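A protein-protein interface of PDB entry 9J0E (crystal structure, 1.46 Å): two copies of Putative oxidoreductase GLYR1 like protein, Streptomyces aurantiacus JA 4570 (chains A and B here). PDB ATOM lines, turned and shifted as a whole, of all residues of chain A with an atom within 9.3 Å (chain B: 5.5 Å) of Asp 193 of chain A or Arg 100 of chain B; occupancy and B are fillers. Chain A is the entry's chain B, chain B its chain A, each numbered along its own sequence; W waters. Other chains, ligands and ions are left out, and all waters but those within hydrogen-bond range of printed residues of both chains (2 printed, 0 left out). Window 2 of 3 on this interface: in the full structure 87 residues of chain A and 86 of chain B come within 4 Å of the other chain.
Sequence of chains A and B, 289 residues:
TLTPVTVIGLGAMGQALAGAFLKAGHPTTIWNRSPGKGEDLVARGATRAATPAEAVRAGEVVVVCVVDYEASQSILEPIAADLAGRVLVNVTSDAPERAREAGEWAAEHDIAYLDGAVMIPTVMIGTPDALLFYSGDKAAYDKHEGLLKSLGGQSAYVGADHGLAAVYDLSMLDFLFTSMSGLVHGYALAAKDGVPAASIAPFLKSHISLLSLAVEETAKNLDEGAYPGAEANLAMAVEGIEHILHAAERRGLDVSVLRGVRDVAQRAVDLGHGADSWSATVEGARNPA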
ATOM      1  N   GLY A 186     -29.682  16.603   6.962  1.00  0.00           N
ATOM      2  CA  GLY A 186     -28.655  17.391   6.304  1.00  0.00           C
ATOM      3  C   GLY A 186     -27.675  17.987   7.293  1.00  0.00           C
ATOM      4  O   GLY A 186     -26.466  18.018   7.051  1.00  0.00           O
ATOM      5  N   TYR A 187     -28.178  18.475   8.421  1.00  0.00           N
ATOM      6  CA  TYR A 187     -27.265  18.962   9.447  1.00  0.00           C
ATOM      7  C   TYR A 187     -26.405  17.827   9.982  1.00  0.00           C
ATOM      8  O   TYR A 187     -25.211  18.011  10.243  1.00  0.00           O
ATOM      9  CB  TYR A 187     -28.074  19.587  10.577  1.00  0.00           C
ATOM     10  CG  TYR A 187     -28.624  20.983  10.340  1.00  0.00           C
ATOM     11  CD1 TYR A 187     -27.972  21.904   9.527  1.00  0.00           C
ATOM     12  CD2 TYR A 187     -29.787  21.385  10.980  1.00  0.00           C
ATOM     13  CE1 TYR A 187     -28.476  23.196   9.362  1.00  0.00           C
ATOM     14  CE2 TYR A 187     -30.296  22.650  10.811  1.00  0.00           C
ATOM     15  CZ  TYR A 187     -29.645  23.557  10.017  1.00  0.00           C
ATOM     16  OH  TYR A 187     -30.152  24.831   9.856  1.00  0.00           O
ATOM     17  N   ALA A 188     -26.990  16.637  10.146  1.00  0.00           N
ATOM     18  CA  ALA A 188     -26.207  15.508  10.622  1.00  0.00           C
ATOM     19  C   ALA A 188     -25.103  15.165   9.632  1.00  0.00           C
ATOM     20  O   ALA A 188     -23.972  14.860  10.028  1.00  0.00           O
ATOM     21  CB  ALA A 188     -27.120  14.310  10.875  1.00  0.00           C
ATOM     22  N   LEU A 189     -25.415  15.206   8.336  1.00  0.00           N
ATOM     23  CA  LEU A 189     -24.401  14.939   7.321  1.00  0.00           C
ATOM     24  C   LEU A 189     -23.252  15.940   7.429  1.00  0.00           C
ATOM     25  O   LEU A 189     -22.070  15.559   7.426  1.00  0.00           O
ATOM     26  CB  LEU A 189     -25.053  14.984   5.939  1.00  0.00           C
ATOM     27  CG  LEU A 189     -24.139  14.674   4.755  1.00  0.00           C
ATOM     28  CD1 LEU A 189     -23.447  13.317   4.932  1.00  0.00           C
ATOM     29  CD2 LEU A 189     -24.965  14.681   3.469  1.00  0.00           C
ATOM     30  N   ALA A 190     -23.581  17.231   7.537  1.00  0.00           N
ATOM     31  CA  ALA A 190     -22.544  18.253   7.649  1.00  0.00           C
ATOM     32  C   ALA A 190     -21.655  18.008   8.866  1.00  0.00           C
ATOM     33  O   ALA A 190     -20.422  18.125   8.786  1.00  0.00           O
ATOM     34  CB  ALA A 190     -23.194  19.637   7.727  1.00  0.00           C
ATOM     35  N   ALA A 191     -22.261  17.663  10.003  1.00  0.00           N
ATOM     36  CA  ALA A 191     -21.491  17.471  11.227  1.00  0.00           C
ATOM     37  C   ALA A 191     -20.518  16.304  11.114  1.00  0.00           C
ATOM     38  O   ALA A 191     -19.474  16.306  11.780  1.00  0.00           O
ATOM     39  CB  ALA A 191     -22.443  17.268  12.407  1.00  0.00           C
ATOM     40  N   LYS A 192     -20.815  15.316  10.265  1.00  0.00           N
ATOM     41  CA  LYS A 192     -19.894  14.199  10.078  1.00  0.00           C
ATOM     42  C   LYS A 192     -18.565  14.632   9.480  1.00  0.00           C
ATOM     43  O   LYS A 192     -17.568  13.915   9.629  1.00  0.00           O
ATOM     44  CB  LYS A 192     -20.545  13.122   9.203  1.00  0.00           C
ATOM     45  CG  LYS A 192     -21.650  12.365   9.907  1.00  0.00           C
ATOM     46  CD  LYS A 192     -21.119  11.440  10.987  1.00  0.00           C
ATOM     47  CE  LYS A 192     -22.235  10.577  11.575  1.00  0.00           C
ATOM     48  NZ  LYS A 192     -21.723   9.705  12.668  1.00  0.00           N
ATOM     49  N   ASP A 193     -18.521  15.782   8.807  1.00  0.00           N
ATOM     50  CA  ASP A 193     -17.280  16.340   8.288  1.00  0.00           C
ATOM     51  C   ASP A 193     -16.864  17.585   9.056  1.00  0.00           C
ATOM     52  O   ASP A 193     -16.113  18.419   8.537  1.00  0.00           O
ATOM     53  CB  ASP A 193     -17.388  16.612   6.789  1.00  0.00           C
ATOM     54  CG  ASP A 193     -17.053  15.394   5.968  1.00  0.00           C
ATOM     55  OD1 ASP A 193     -15.871  14.989   5.957  1.00  0.00           O
ATOM     56  OD2 ASP A 193     -17.963  14.824   5.359  1.00  0.00           O
ATOM     57  N   GLY A 194     -17.349  17.726  10.285  1.00  0.00           N
ATOM     58  CA  GLY A 194     -16.914  18.800  11.151  1.00  0.00           C
ATOM     59  C   GLY A 194     -17.547  20.147  10.895  1.00  0.00           C
ATOM     60  O   GLY A 194     -17.082  21.139  11.456  1.00  0.00           O
ATOM     61  N   VAL A 195     -18.599  20.230  10.084  1.00  0.00           N
ATOM     62  CA  VAL A 195     -19.215  21.512   9.752  1.00  0.00           C
ATOM     63  C   VAL A 195     -20.414  21.716  10.674  1.00  0.00           C
ATOM     64  O   VAL A 195     -21.397  20.959  10.578  1.00  0.00           O
ATOM     65  CB  VAL A 195     -19.609  21.599   8.270  1.00  0.00           C
ATOM     66  CG1 VAL A 195     -20.345  22.907   8.019  1.00  0.00           C
ATOM     67  CG2 VAL A 195     -18.366  21.503   7.366  1.00  0.00           C
ATOM     68  N   PRO A 196     -20.387  22.697  11.570  1.00  0.00           N
ATOM     69  CA  PRO A 196     -21.516  22.902  12.484  1.00  0.00           C
ATOM     70  C   PRO A 196     -22.774  23.314  11.741  1.00  0.00           C
ATOM     71  O   PRO A 196     -22.730  23.917  10.664  1.00  0.00           O
ATOM     72  CB  PRO A 196     -21.039  24.042  13.389  1.00  0.00           C
ATOM     73  CG  PRO A 196     -19.539  24.046  13.260  1.00  0.00           C
ATOM     74  CD  PRO A 196     -19.259  23.596  11.859  1.00  0.00           C
ATOM     75  N   ILE A 200     -24.102  25.903   8.243  1.00  0.00           N
ATOM     76  CA  ILE A 200     -25.013  25.589   7.140  1.00  0.00           C
ATOM     77  C   ILE A 200     -26.210  26.534   7.142  1.00  0.00           C
ATOM     78  O   ILE A 200     -26.680  26.964   6.082  1.00  0.00           O
ATOM     79  CB  ILE A 200     -25.482  24.121   7.239  1.00  0.00           C
ATOM     80  CG1 ILE A 200     -24.314  23.120   7.181  1.00  0.00           C
ATOM     81  CG2 ILE A 200     -26.523  23.810   6.149  1.00  0.00           C
ATOM     82  CD1 ILE A 200     -23.578  23.064   5.846  1.00  0.00           C
ATOM     83  N   ALA A 247     -22.827   9.105   0.493  1.00  0.00           N
ATOM     84  CA  ALA A 247     -22.028   9.877   1.443  1.00  0.00           C
ATOM     85  C   ALA A 247     -22.527   9.675   2.871  1.00  0.00           C
ATOM     86  O   ALA A 247     -21.738   9.446   3.798  1.00  0.00           O
ATOM     87  CB  ALA A 247     -22.034  11.356   1.058  1.00  0.00           C
ATOM     88  N   ALA A 248     -23.845   9.735   3.069  1.00  0.00           N
ATOM     89  CA  ALA A 248     -24.384   9.600   4.418  1.00  0.00           C
ATOM     90  C   ALA A 248     -24.190   8.186   4.956  1.00  0.00           C
ATOM     91  O   ALA A 248     -23.810   8.003   6.119  1.00  0.00           O
ATOM     92  CB  ALA A 248     -25.865   9.991   4.421  1.00  0.00           C
ATOM     93  N   ARG A 250     -21.936   6.006   4.272  1.00  0.00           N
ATOM     94  CA  ARG A 250     -20.525   5.744   4.512  1.00  0.00           C
ATOM     95  C   ARG A 250     -20.039   6.448   5.790  1.00  0.00           C
ATOM     96  O   ARG A 250     -18.972   6.119   6.325  1.00  0.00           O
ATOM     97  CB  ARG A 250     -19.745   6.242   3.280  1.00  0.00           C
ATOM     98  CG  ARG A 250     -19.795   5.534   2.031  1.00  0.00           C
ATOM     99  CD  ARG A 250     -21.190   5.213   1.550  1.00  0.00           C
ATOM    100  NE  ARG A 250     -21.117   4.123   0.606  1.00  0.00           N
ATOM    101  CZ  ARG A 250     -20.551   4.192  -0.589  1.00  0.00           C
ATOM    102  NH1 ARG A 250     -19.802   5.215  -0.944  1.00  0.00           N
ATOM    103  NH2 ARG A 250     -20.814   3.250  -1.490  1.00  0.00           N
ATOM    104  N   ARG A 251     -20.796   7.429   6.271  1.00  0.00           N
ATOM    105  CA  ARG A 251     -20.527   8.129   7.513  1.00  0.00           C
ATOM    106  C   ARG A 251     -21.326   7.551   8.670  1.00  0.00           C
ATOM    107  O   ARG A 251     -21.285   8.101   9.776  1.00  0.00           O
ATOM    108  CB  ARG A 251     -20.816   9.620   7.328  1.00  0.00           C
ATOM    109  CG  ARG A 251     -19.798  10.315   6.420  1.00  0.00           C
ATOM    110  CD  ARG A 251     -20.328  11.603   5.803  1.00  0.00           C
ATOM    111  NE  ARG A 251     -19.273  12.322   5.097  1.00  0.00           N
ATOM    112  CZ  ARG A 251     -18.774  11.950   3.924  1.00  0.00           C
ATOM    113  NH1 ARG A 251     -19.236  10.894   3.282  1.00  0.00           N
ATOM    114  NH2 ARG A 251     -17.781  12.654   3.387  1.00  0.00           N
ATOM    115  N   LEU A 253     -24.713   7.108   8.957  1.00  0.00           N
ATOM    116  CA  LEU A 253     -26.055   7.612   9.223  1.00  0.00           C
ATOM    117  C   LEU A 253     -27.110   6.651   8.689  1.00  0.00           C
ATOM    118  O   LEU A 253     -26.892   5.929   7.712  1.00  0.00           O
ATOM    119  CB  LEU A 253     -26.244   8.978   8.567  1.00  0.00           C
ATOM    120  CG  LEU A 253     -25.407  10.123   9.122  1.00  0.00           C
ATOM    121  CD1 LEU A 253     -25.588  11.357   8.244  1.00  0.00           C
ATOM    122  CD2 LEU A 253     -25.781  10.430  10.579  1.00  0.00           C
ATOM    123  N   ALA B  95     -19.844  13.686  -3.881  1.00  0.00           N
ATOM    124  CA  ALA B  95     -19.489  13.491  -2.482  1.00  0.00           C
ATOM    125  C   ALA B  95     -18.155  14.155  -2.143  1.00  0.00           C
ATOM    126  O   ALA B  95     -17.284  14.308  -3.010  1.00  0.00           O
ATOM    127  CB  ALA B  95     -19.387  12.000  -2.182  1.00  0.00           C
ATOM    128  N   PRO B  96     -17.967  14.551  -0.879  1.00  0.00           N
ATOM    129  CA  PRO B  96     -16.664  15.110  -0.481  1.00  0.00           C
ATOM    130  C   PRO B  96     -15.498  14.193  -0.801  1.00  0.00           C
ATOM    131  O   PRO B  96     -14.409  14.693  -1.124  1.00  0.00           O
ATOM    132  CB  PRO B  96     -16.818  15.309   1.031  1.00  0.00           C
ATOM    133  CG  PRO B  96     -18.323  15.513   1.225  1.00  0.00           C
ATOM    134  CD  PRO B  96     -18.942  14.567   0.235  1.00  0.00           C
ATOM    135  N   GLU B  97     -15.687  12.871  -0.705  1.00  0.00           N
ATOM    136  CA  GLU B  97     -14.605  11.939  -1.021  1.00  0.00           C
ATOM    137  C   GLU B  97     -14.144  12.097  -2.466  1.00  0.00           C
ATOM    138  O   GLU B  97     -12.942  12.001  -2.757  1.00  0.00           O
ATOM    139  CB  GLU B  97     -15.047  10.493  -0.782  1.00  0.00           C
ATOM    140  CG  GLU B  97     -15.608  10.171   0.596  1.00  0.00           C
ATOM    141  CD  GLU B  97     -17.111  10.381   0.679  1.00  0.00           C
ATOM    142  OE1 GLU B  97     -17.538  11.539   0.604  1.00  0.00           O
ATOM    143  OE2 GLU B  97     -17.864   9.392   0.807  1.00  0.00           O
ATOM    144  N   ARG B  98     -15.085  12.309  -3.391  1.00  0.00           N
ATOM    145  CA  ARG B  98     -14.711  12.482  -4.792  1.00  0.00           C
ATOM    146  C   ARG B  98     -14.001  13.811  -5.005  1.00  0.00           C
ATOM    147  O   ARG B  98     -13.022  13.888  -5.758  1.00  0.00           O
ATOM    148  CB  ARG B  98     -15.948  12.396  -5.689  1.00  0.00           C
ATOM    149  CG  ARG B  98     -16.725  11.083  -5.599  1.00  0.00           C
ATOM    150  CD  ARG B  98     -15.955   9.911  -6.202  1.00  0.00           C
ATOM    151  NE  ARG B  98     -15.164   9.220  -5.190  1.00  0.00           N
ATOM    152  CZ  ARG B  98     -15.681   8.509  -4.194  1.00  0.00           C
ATOM    153  NH1 ARG B  98     -16.991   8.390  -4.033  1.00  0.00           N
ATOM    154  NH2 ARG B  98     -14.864   7.907  -3.335  1.00  0.00           N
ATOM    155  N   ALA B  99     -14.474  14.871  -4.343  1.00  0.00           N
ATOM    156  CA  ALA B  99     -13.815  16.164  -4.460  1.00  0.00           C
ATOM    157  C   ALA B  99     -12.394  16.107  -3.923  1.00  0.00           C
ATOM    158  O   ALA B  99     -11.478  16.710  -4.493  1.00  0.00           O
ATOM    159  CB  ALA B  99     -14.618  17.225  -3.697  1.00  0.00           C
ATOM    160  N   ARG B 100     -12.196  15.383  -2.822  1.00  0.00           N
ATOM    161  CA  ARG B 100     -10.873  15.292  -2.218  1.00  0.00           C
ATOM    162  C   ARG B 100      -9.925  14.476  -3.088  1.00  0.00           C
ATOM    163  O   ARG B 100      -8.747  14.834  -3.230  1.00  0.00           O
ATOM    164  CB  ARG B 100     -10.998  14.740  -0.796  1.00  0.00           C
ATOM    165  CG  ARG B 100     -11.639  15.775   0.143  1.00  0.00           C
ATOM    166  CD  ARG B 100     -12.072  15.248   1.500  1.00  0.00           C
ATOM    167  NE  ARG B 100     -12.422  16.382   2.349  1.00  0.00           N
ATOM    168  CZ  ARG B 100     -13.355  16.381   3.295  1.00  0.00           C
ATOM    169  NH1 ARG B 100     -14.081  15.305   3.552  1.00  0.00           N
ATOM    170  NH2 ARG B 100     -13.568  17.493   3.996  1.00  0.00           N
ATOM    171  N   GLU B 101     -10.425  13.402  -3.704  1.00  0.00           N
ATOM    172  CA  GLU B 101      -9.610  12.655  -4.660  1.00  0.00           C
ATOM    173  C   GLU B 101      -9.232  13.531  -5.848  1.00  0.00           C
ATOM    174  O   GLU B 101      -8.075  13.539  -6.290  1.00  0.00           O
ATOM    175  CB  GLU B 101     -10.367  11.421  -5.142  1.00  0.00           C
ATOM    176  CG  GLU B 101     -10.651  10.392  -4.082  1.00  0.00           C
ATOM    177  CD  GLU B 101     -11.367   9.186  -4.652  1.00  0.00           C
ATOM    178  OE1 GLU B 101     -10.711   8.386  -5.359  1.00  0.00           O
ATOM    179  OE2 GLU B 101     -12.591   9.052  -4.423  1.00  0.00           O
ATOM    180  N   ALA B 102     -10.200  14.275  -6.387  1.00  0.00           N
ATOM    181  CA  ALA B 102      -9.890  15.167  -7.499  1.00  0.00           C
ATOM    182  C   ALA B 102      -8.880  16.223  -7.080  1.00  0.00           C
ATOM    183  O   ALA B 102      -7.984  16.587  -7.854  1.00  0.00           O
ATOM    184  CB  ALA B 102     -11.168  15.816  -8.030  1.00  0.00           C
ATOM    185  N   GLY B 103      -9.006  16.731  -5.853  1.00  0.00           N
ATOM    186  CA  GLY B 103      -8.051  17.717  -5.377  1.00  0.00           C
ATOM    187  C   GLY B 103      -6.646  17.158  -5.248  1.00  0.00           C
ATOM    188  O   GLY B 103      -5.668  17.850  -5.532  1.00  0.00           O
ATOM    189  N   GLU B 104      -6.526  15.906  -4.805  1.00  0.00           N
ATOM    190  CA  GLU B 104      -5.205  15.285  -4.731  1.00  0.00           C
ATOM    191  C   GLU B 104      -4.609  15.104  -6.120  1.00  0.00           C
ATOM    192  O   GLU B 104      -3.408  15.323  -6.321  1.00  0.00           O
ATOM    193  CB  GLU B 104      -5.290  13.954  -3.989  1.00  0.00           C
ATOM    194  CG  GLU B 104      -5.383  14.125  -2.482  1.00  0.00           C
ATOM    195  CD  GLU B 104      -5.846  12.873  -1.765  1.00  0.00           C
ATOM    196  OE1 GLU B 104      -6.635  13.001  -0.799  1.00  0.00           O
ATOM    197  OE2 GLU B 104      -5.430  11.767  -2.169  1.00  0.00           O
ATOM    198  N   TRP B 105      -5.438  14.713  -7.089  1.00  0.00           N
ATOM    199  CA  TRP B 105      -4.967  14.578  -8.462  1.00  0.00           C
ATOM    200  C   TRP B 105      -4.532  15.924  -9.025  1.00  0.00           C
ATOM    201  O   TRP B 105      -3.488  16.028  -9.679  1.00  0.00           O
ATOM    202  CB  TRP B 105      -6.081  13.969  -9.308  1.00  0.00           C
ATOM    203  CG  TRP B 105      -5.918  14.180 -10.779  1.00  0.00           C
ATOM    204  CD1 TRP B 105      -5.194  13.412 -11.645  1.00  0.00           C
ATOM    205  CD2 TRP B 105      -6.500  15.230 -11.559  1.00  0.00           C
ATOM    206  NE1 TRP B 105      -5.287  13.922 -12.918  1.00  0.00           N
ATOM    207  CE2 TRP B 105      -6.081  15.040 -12.893  1.00  0.00           C
ATOM    208  CE3 TRP B 105      -7.337  16.313 -11.258  1.00  0.00           C
ATOM    209  CZ2 TRP B 105      -6.472  15.895 -13.928  1.00  0.00           C
ATOM    210  CZ3 TRP B 105      -7.723  17.159 -12.284  1.00  0.00           C
ATOM    211  CH2 TRP B 105      -7.288  16.947 -13.603  1.00  0.00           C
ATOM    212  N   ASP B 161      -9.874  23.304   2.337  1.00  0.00           N
ATOM    213  CA  ASP B 161      -9.987  21.866   2.135  1.00  0.00           C
ATOM    214  C   ASP B 161     -10.884  21.594   0.934  1.00  0.00           C
ATOM    215  O   ASP B 161     -11.996  22.117   0.845  1.00  0.00           O
ATOM    216  CB  ASP B 161     -10.571  21.216   3.391  1.00  0.00           C
ATOM    217  CG  ASP B 161     -10.651  19.704   3.281  1.00  0.00           C
ATOM    218  OD1 ASP B 161     -11.562  19.195   2.591  1.00  0.00           O
ATOM    219  OD2 ASP B 161      -9.783  19.019   3.861  1.00  0.00           O
ATOM    220  N   HIS B 162     -10.398  20.774   0.003  1.00  0.00           N
ATOM    221  CA  HIS B 162     -11.089  20.646  -1.275  1.00  0.00           C
ATOM    222  C   HIS B 162     -12.438  19.941  -1.178  1.00  0.00           C
ATOM    223  O   HIS B 162     -13.199  19.986  -2.148  1.00  0.00           O
ATOM    224  CB  HIS B 162     -10.189  19.976  -2.317  1.00  0.00           C
ATOM    225  CG  HIS B 162      -9.070  20.852  -2.798  1.00  0.00           C
ATOM    226  ND1 HIS B 162      -9.254  21.857  -3.724  1.00  0.00           N
ATOM    227  CD2 HIS B 162      -7.757  20.879  -2.473  1.00  0.00           C
ATOM    228  CE1 HIS B 162      -8.101  22.462  -3.952  1.00  0.00           C
ATOM    229  NE2 HIS B 162      -7.176  21.888  -3.205  1.00  0.00           N
ATOM    230  N   GLY B 163     -12.759  19.304  -0.051  1.00  0.00           N
ATOM    231  CA  GLY B 163     -14.056  18.673   0.102  1.00  0.00           C
ATOM    232  C   GLY B 163     -15.127  19.529   0.744  1.00  0.00           C
ATOM    233  O   GLY B 163     -16.286  19.113   0.804  1.00  0.00           O
ATOM    234  N   LEU B 164     -14.785  20.731   1.213  1.00  0.00           N
ATOM    235  CA  LEU B 164     -15.739  21.478   2.029  1.00  0.00           C
ATOM    236  C   LEU B 164     -16.958  21.933   1.231  1.00  0.00           C
ATOM    237  O   LEU B 164     -18.081  21.905   1.748  1.00  0.00           O
ATOM    238  CB  LEU B 164     -15.055  22.658   2.714  1.00  0.00           C
ATOM    239  CG  LEU B 164     -14.273  22.271   3.965  1.00  0.00           C
ATOM    240  CD1 LEU B 164     -13.400  23.435   4.411  1.00  0.00           C
ATOM    241  CD2 LEU B 164     -15.213  21.824   5.074  1.00  0.00           C
ATOM    242  N   VAL B 167     -19.392  19.243   1.166  1.00  0.00           N
ATOM    243  CA  VAL B 167     -20.082  19.043   2.439  1.00  0.00           C
ATOM    244  C   VAL B 167     -21.297  19.959   2.533  1.00  0.00           C
ATOM    245  O   VAL B 167     -22.402  19.525   2.875  1.00  0.00           O
ATOM    246  CB  VAL B 167     -19.125  19.258   3.626  1.00  0.00           C
ATOM    247  CG1 VAL B 167     -19.897  19.134   4.936  1.00  0.00           C
ATOM    248  CG2 VAL B 167     -17.964  18.274   3.595  1.00  0.00           C
HETATM  249  O   HOH W   1     -19.323   8.362  -0.884  1.00  0.00           O
HETATM  250  O   HOH W   2     -14.211  18.206   6.599  1.00  0.00           O
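The side-chain carboxylate of Glu 97 of chain B lies within salt-bridge range of the guanidinium group of Arg 251 of chain A (3.0 Å).
NH1 of Arg 100 of chain B lies within salt-bridge range of OD1 of Asp 193 of chain A, at 3.0 Å.
The backbone carbonyl oxygen of Ala 247 of chain A sits at hydrogen-bond distance from the guanidinium group of Arg 251 of chain A, at 2.9 Å.
The backbone carbonyl oxygen of Arg 251 of chain A lies close to the side-chain amino group of Lys 192 of chain A (3.3 Å).
O of Ala 190 of chain A sits at hydrogen-bond distance from N of Val 195 of chain A, at 3.1 Å.
OD1 of Asp 161 of chain B is in salt-bridge range of NE of Arg 100 of chain B.
The side-chain carboxylate (OD2) of Asp 193 of chain A lies within salt-bridge range of the guanidinium group (NE) of Arg 251 of chain A (2.8 Å).
Among the printed residues, pairs that only touch across the chains: Ala 190 of chain A with Val 167 of chain B, Asp 193 of chain A with Val 167 of chain B, Val 195 of chain A with Leu 164 of chain B, Val 195 of chain A with Val 167 of chain B and Arg 251 of chain A with Pro 96 of chain B.
Asp 193 of chain A touches just these residues of chain B: Arg 100 and Val 167.
Printed residues of chain A within 4 Å of Pro 96 of chain B: Arg 251.
Of the printed residues of chain A, Glu 97 of chain B touches Arg 251.
No residue of chain A comes within 4 Å of Ala 99 of chain B.
Arg 100 of chain B touches just one residue of chain A: Asp 193.
Gly 103 of chain B touches none of the printed residues of chain A.
Of the printed residues of chain A, Leu 164 of chain B touches Val 195.
Printed residues of chain A within 4 Å of Val 167 of chain B: Ala 190 (3.9 Å), Asp 193 (3.6 Å) and Val 195 (3.7 Å).
The nearest residue of chain A that does not touch Arg 100 of chain B is Arg 251 of chain A (4.6 Å).
Printed residues of chain A that touch a printed residue of chain B: Ala 190, Asp 193, Val 195 and Arg 251.
Along chain A the printed residues that touch a printed residue of chain B span positions 190 to 251.
Among the printed residues, 7 pairs touch across the chains.
No position is printed for both chains.
Of the 7 pairs that touch across the chains among the printed residues, none has its exchanged pair printed and touching as well.
Water W1 bridges OE2 of Glu 97 of chain B and NH1 of Arg 250 of chain A.
Water W2 bridges O of Asp 193 of chain A (2.7 Å) and NH2 of Arg 100 of chain B (2.8 Å).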
